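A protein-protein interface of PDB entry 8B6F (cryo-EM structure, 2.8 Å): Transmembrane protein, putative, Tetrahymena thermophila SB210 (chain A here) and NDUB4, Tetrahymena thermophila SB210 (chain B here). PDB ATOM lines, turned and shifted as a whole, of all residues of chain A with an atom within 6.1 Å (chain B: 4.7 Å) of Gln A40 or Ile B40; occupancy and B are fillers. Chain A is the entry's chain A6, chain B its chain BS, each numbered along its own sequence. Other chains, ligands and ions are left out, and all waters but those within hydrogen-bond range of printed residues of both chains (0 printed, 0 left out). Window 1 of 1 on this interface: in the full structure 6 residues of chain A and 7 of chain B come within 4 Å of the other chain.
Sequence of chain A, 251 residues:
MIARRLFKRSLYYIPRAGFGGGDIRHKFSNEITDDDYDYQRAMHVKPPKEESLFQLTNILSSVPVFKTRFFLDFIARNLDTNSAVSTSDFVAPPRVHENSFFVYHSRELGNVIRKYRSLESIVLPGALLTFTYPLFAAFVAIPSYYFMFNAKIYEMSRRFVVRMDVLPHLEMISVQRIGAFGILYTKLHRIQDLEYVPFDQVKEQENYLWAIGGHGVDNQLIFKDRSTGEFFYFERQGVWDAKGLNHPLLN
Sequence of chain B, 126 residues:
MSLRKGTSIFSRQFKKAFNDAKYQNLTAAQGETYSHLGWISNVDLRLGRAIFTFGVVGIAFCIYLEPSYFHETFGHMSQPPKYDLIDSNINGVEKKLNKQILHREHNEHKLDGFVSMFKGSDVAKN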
ATOM      1  N   ASP A  36     -19.911  10.838  19.529  1.00  0.00           N
ATOM      2  CA  ASP A  36     -19.423   9.605  18.923  1.00  0.00           C
ATOM      3  C   ASP A  36     -18.034   9.779  18.324  1.00  0.00           C
ATOM      4  O   ASP A  36     -17.276   8.807  18.249  1.00  0.00           O
ATOM      5  CB  ASP A  36     -20.394   9.126  17.843  1.00  0.00           C
ATOM      6  CG  ASP A  36     -21.762   8.783  18.398  1.00  0.00           C
ATOM      7  OD1 ASP A  36     -21.950   8.892  19.627  1.00  0.00           O
ATOM      8  OD2 ASP A  36     -22.648   8.401  17.606  1.00  0.00           O
ATOM      9  N   TYR A  37     -17.688  10.989  17.889  1.00  0.00           N
ATOM     10  CA  TYR A  37     -16.375  11.258  17.316  1.00  0.00           C
ATOM     11  C   TYR A  37     -15.313  11.562  18.364  1.00  0.00           C
ATOM     12  O   TYR A  37     -14.132  11.640  18.013  1.00  0.00           O
ATOM     13  CB  TYR A  37     -16.456  12.438  16.340  1.00  0.00           C
ATOM     14  CG  TYR A  37     -16.928  12.087  14.944  1.00  0.00           C
ATOM     15  CD1 TYR A  37     -16.408  10.996  14.263  1.00  0.00           C
ATOM     16  CD2 TYR A  37     -17.887  12.861  14.306  1.00  0.00           C
ATOM     17  CE1 TYR A  37     -16.835  10.682  12.989  1.00  0.00           C
ATOM     18  CE2 TYR A  37     -18.319  12.556  13.032  1.00  0.00           C
ATOM     19  CZ  TYR A  37     -17.789  11.467  12.379  1.00  0.00           C
ATOM     20  OH  TYR A  37     -18.218  11.158  11.110  1.00  0.00           O
ATOM     21  N   ASP A  38     -15.697  11.751  19.628  1.00  0.00           N
ATOM     22  CA  ASP A  38     -14.716  12.095  20.652  1.00  0.00           C
ATOM     23  C   ASP A  38     -13.577  11.084  20.724  1.00  0.00           C
ATOM     24  O   ASP A  38     -12.452  11.446  21.084  1.00  0.00           O
ATOM     25  CB  ASP A  38     -15.395  12.205  22.018  1.00  0.00           C
ATOM     26  CG  ASP A  38     -16.238  13.457  22.151  1.00  0.00           C
ATOM     27  OD1 ASP A  38     -15.953  14.447  21.445  1.00  0.00           O
ATOM     28  OD2 ASP A  38     -17.183  13.453  22.967  1.00  0.00           O
ATOM     29  N   TYR A  39     -13.840   9.819  20.392  1.00  0.00           N
ATOM     30  CA  TYR A  39     -12.795   8.808  20.495  1.00  0.00           C
ATOM     31  C   TYR A  39     -11.663   9.041  19.505  1.00  0.00           C
ATOM     32  O   TYR A  39     -10.582   8.469  19.676  1.00  0.00           O
ATOM     33  CB  TYR A  39     -13.381   7.413  20.283  1.00  0.00           C
ATOM     34  CG  TYR A  39     -13.582   7.043  18.835  1.00  0.00           C
ATOM     35  CD1 TYR A  39     -14.624   7.584  18.098  1.00  0.00           C
ATOM     36  CD2 TYR A  39     -12.736   6.138  18.210  1.00  0.00           C
ATOM     37  CE1 TYR A  39     -14.815   7.244  16.775  1.00  0.00           C
ATOM     38  CE2 TYR A  39     -12.919   5.791  16.888  1.00  0.00           C
ATOM     39  CZ  TYR A  39     -13.961   6.347  16.177  1.00  0.00           C
ATOM     40  OH  TYR A  39     -14.147   6.006  14.859  1.00  0.00           O
ATOM     41  N   GLN A  40     -11.882   9.862  18.479  1.00  0.00           N
ATOM     42  CA  GLN A  40     -10.848  10.155  17.496  1.00  0.00           C
ATOM     43  C   GLN A  40      -9.893  11.248  17.947  1.00  0.00           C
ATOM     44  O   GLN A  40      -8.921  11.527  17.239  1.00  0.00           O
ATOM     45  CB  GLN A  40     -11.487  10.561  16.167  1.00  0.00           C
ATOM     46  CG  GLN A  40     -12.380   9.496  15.567  1.00  0.00           C
ATOM     47  CD  GLN A  40     -12.858   9.859  14.180  1.00  0.00           C
ATOM     48  OE1 GLN A  40     -12.684  10.990  13.729  1.00  0.00           O
ATOM     49  NE2 GLN A  40     -13.460   8.899  13.488  1.00  0.00           N
ATOM     50  N   ARG A  41     -10.140  11.876  19.098  1.00  0.00           N
ATOM     51  CA  ARG A  41      -9.260  12.942  19.558  1.00  0.00           C
ATOM     52  C   ARG A  41      -7.843  12.448  19.805  1.00  0.00           C
ATOM     53  O   ARG A  41      -6.905  13.251  19.776  1.00  0.00           O
ATOM     54  CB  ARG A  41      -9.825  13.577  20.827  1.00  0.00           C
ATOM     55  CG  ARG A  41     -11.059  14.425  20.580  1.00  0.00           C
ATOM     56  CD  ARG A  41     -11.582  15.035  21.866  1.00  0.00           C
ATOM     57  NE  ARG A  41     -12.580  16.066  21.606  1.00  0.00           N
ATOM     58  CZ  ARG A  41     -12.302  17.344  21.387  1.00  0.00           C
ATOM     59  NH1 ARG A  41     -11.058  17.793  21.392  1.00  0.00           N
ATOM     60  NH2 ARG A  41     -13.298  18.194  21.159  1.00  0.00           N
ATOM     61  N   ALA A  42      -7.664  11.152  20.059  1.00  0.00           N
ATOM     62  CA  ALA A  42      -6.318  10.607  20.184  1.00  0.00           C
ATOM     63  C   ALA A  42      -5.574  10.684  18.856  1.00  0.00           C
ATOM     64  O   ALA A  42      -4.408  11.091  18.810  1.00  0.00           O
ATOM     65  CB  ALA A  42      -6.382   9.166  20.686  1.00  0.00           C
ATOM     66  N   MET A  43      -6.235  10.298  17.764  1.00  0.00           N
ATOM     67  CA  MET A  43      -5.633  10.335  16.437  1.00  0.00           C
ATOM     68  C   MET A  43      -5.925  11.622  15.678  1.00  0.00           C
ATOM     69  O   MET A  43      -5.351  11.829  14.605  1.00  0.00           O
ATOM     70  CB  MET A  43      -6.124   9.149  15.597  1.00  0.00           C
ATOM     71  CG  MET A  43      -5.654   7.788  16.089  1.00  0.00           C
ATOM     72  SD  MET A  43      -6.425   7.268  17.632  1.00  0.00           S
ATOM     73  CE  MET A  43      -8.125   7.052  17.114  1.00  0.00           C
ATOM     74  N   HIS A  44      -6.791  12.487  16.201  1.00  0.00           N
ATOM     75  CA  HIS A  44      -7.172  13.722  15.531  1.00  0.00           C
ATOM     76  C   HIS A  44      -7.004  14.888  16.491  1.00  0.00           C
ATOM     77  O   HIS A  44      -7.349  14.784  17.672  1.00  0.00           O
ATOM     78  CB  HIS A  44      -8.619  13.653  15.030  1.00  0.00           C
ATOM     79  CG  HIS A  44      -8.924  14.612  13.921  1.00  0.00           C
ATOM     80  ND1 HIS A  44     -10.172  14.704  13.343  1.00  0.00           N
ATOM     81  CD2 HIS A  44      -8.145  15.513  13.277  1.00  0.00           C
ATOM     82  CE1 HIS A  44     -10.149  15.622  12.394  1.00  0.00           C
ATOM     83  NE2 HIS A  44      -8.930  16.128  12.333  1.00  0.00           N
ATOM     84  N   VAL A  45      -6.482  15.999  15.982  1.00  0.00           N
ATOM     85  CA  VAL A  45      -6.156  17.157  16.806  1.00  0.00           C
ATOM     86  C   VAL A  45      -7.347  18.110  16.798  1.00  0.00           C
ATOM     87  O   VAL A  45      -7.668  18.712  15.770  1.00  0.00           O
ATOM     88  CB  VAL A  45      -4.883  17.853  16.314  1.00  0.00           C
ATOM     89  CG1 VAL A  45      -4.640  19.151  17.079  1.00  0.00           C
ATOM     90  CG2 VAL A  45      -3.690  16.923  16.452  1.00  0.00           C
ATOM     91  N   TRP B  39     -13.225  15.403  10.150  1.00  0.00           N
ATOM     92  CA  TRP B  39     -13.574  14.153  10.808  1.00  0.00           C
ATOM     93  C   TRP B  39     -12.790  13.031  10.144  1.00  0.00           C
ATOM     94  O   TRP B  39     -11.976  13.263   9.246  1.00  0.00           O
ATOM     95  CB  TRP B  39     -15.081  13.900  10.728  1.00  0.00           C
ATOM     96  CG  TRP B  39     -15.558  13.781   9.319  1.00  0.00           C
ATOM     97  CD1 TRP B  39     -15.777  12.630   8.625  1.00  0.00           C
ATOM     98  CD2 TRP B  39     -15.857  14.856   8.421  1.00  0.00           C
ATOM     99  NE1 TRP B  39     -16.200  12.921   7.352  1.00  0.00           N
ATOM    100  CE2 TRP B  39     -16.256  14.281   7.202  1.00  0.00           C
ATOM    101  CE3 TRP B  39     -15.828  16.249   8.532  1.00  0.00           C
ATOM    102  CZ2 TRP B  39     -16.625  15.048   6.101  1.00  0.00           C
ATOM    103  CZ3 TRP B  39     -16.194  17.008   7.439  1.00  0.00           C
ATOM    104  CH2 TRP B  39     -16.588  16.406   6.239  1.00  0.00           C
ATOM    105  N   ILE B  40     -13.047  11.807  10.591  1.00  0.00           N
ATOM    106  CA  ILE B  40     -12.455  10.614  10.000  1.00  0.00           C
ATOM    107  C   ILE B  40     -13.546   9.560   9.899  1.00  0.00           C
ATOM    108  O   ILE B  40     -14.379   9.426  10.800  1.00  0.00           O
ATOM    109  CB  ILE B  40     -11.257  10.097  10.823  1.00  0.00           C
ATOM    110  CG1 ILE B  40     -10.265  11.239  11.070  1.00  0.00           C
ATOM    111  CG2 ILE B  40     -10.592   8.934  10.102  1.00  0.00           C
ATOM    112  CD1 ILE B  40      -8.961  10.826  11.742  1.00  0.00           C
ATOM    113  N   SER B  41     -13.549   8.823   8.792  1.00  0.00           N
ATOM    114  CA  SER B  41     -14.543   7.781   8.575  1.00  0.00           C
ATOM    115  C   SER B  41     -14.642   6.869   9.789  1.00  0.00           C
ATOM    116  O   SER B  41     -13.670   6.211  10.166  1.00  0.00           O
ATOM    117  CB  SER B  41     -14.182   6.975   7.327  1.00  0.00           C
ATOM    118  OG  SER B  41     -15.059   5.876   7.168  1.00  0.00           O
ATOM    119  N   ASN B  42     -15.826   6.840  10.403  1.00  0.00           N
ATOM    120  CA  ASN B  42     -15.993   6.127  11.665  1.00  0.00           C
ATOM    121  C   ASN B  42     -15.820   4.625  11.480  1.00  0.00           C
ATOM    122  O   ASN B  42     -15.045   3.986  12.201  1.00  0.00           O
ATOM    123  CB  ASN B  42     -17.366   6.441  12.257  1.00  0.00           C
ATOM    124  CG  ASN B  42     -17.549   5.859  13.643  1.00  0.00           C
ATOM    125  OD1 ASN B  42     -17.042   6.397  14.625  1.00  0.00           O
ATOM    126  ND2 ASN B  42     -18.287   4.759  13.731  1.00  0.00           N
ATOM    127  N   LEU B  45     -12.223   3.692  10.357  1.00  0.00           N
ATOM    128  CA  LEU B  45     -11.271   3.812  11.454  1.00  0.00           C
ATOM    129  C   LEU B  45     -11.445   2.682  12.457  1.00  0.00           C
ATOM    130  O   LEU B  45     -10.456   2.129  12.954  1.00  0.00           O
ATOM    131  CB  LEU B  45     -11.432   5.165  12.145  1.00  0.00           C
ATOM    132  CG  LEU B  45     -10.407   5.478  13.239  1.00  0.00           C
ATOM    133  CD1 LEU B  45      -9.006   5.569  12.660  1.00  0.00           C
ATOM    134  CD2 LEU B  45     -10.768   6.758  13.962  1.00  0.00           C
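The backbone carbonyl oxygen (O) of Ile B40 lies within hydrogen-bond range of the side-chain amide nitrogen (NE2) of Gln A40.
The side-chain amide oxygen (OD1) of Asn B42 lies within hydrogen-bond range of the side-chain hydroxyl (OH) of Tyr A39.
Of chain B, only Ile B40 and Leu B45 come within 4 Å of Gln A40.
Ile B40 touches two residues of chain A.
Of the printed residues of chain B, Tyr A39 touches Asn B42 (2.9 Å) and Leu B45 (3.6 Å).
Of the printed residues of chain B, His A44 touches Trp B39 (3.8 Å).
Asp A36 touches none of the printed residues of chain B.
The nearest printed residue of chain B that does not touch Tyr A37 is Asn B42 (4.3 Å).
The side-chain hydroxyl of Tyr A39 lies within hydrogen-bond range of the side-chain amide nitrogen of Gln A40.
Tyr A37 touches Trp B39 (OH to CD1, 3.8 Å).
Tyr A37 touches Ile B40.
Leu B45 touches Tyr A39 (CD2 to OH, 3.6 Å).
Gln A40 touches Leu B45.
N of Trp B39 touches CE1 of His A44, at 3.8 Å.
Of the 10 printed residues of chain A, 4 touch a printed residue of chain B.
Printed residues of chain B that touch a printed residue of chain A: Trp B39, Ile B40, Asn B42 and Leu B45.
Hydrophobic or aromatic side chains of chain B that line the printed part of chain A: Trp B39, Ile B40 and Leu B45.
Among the printed residues, 7 pairs touch across the chains.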
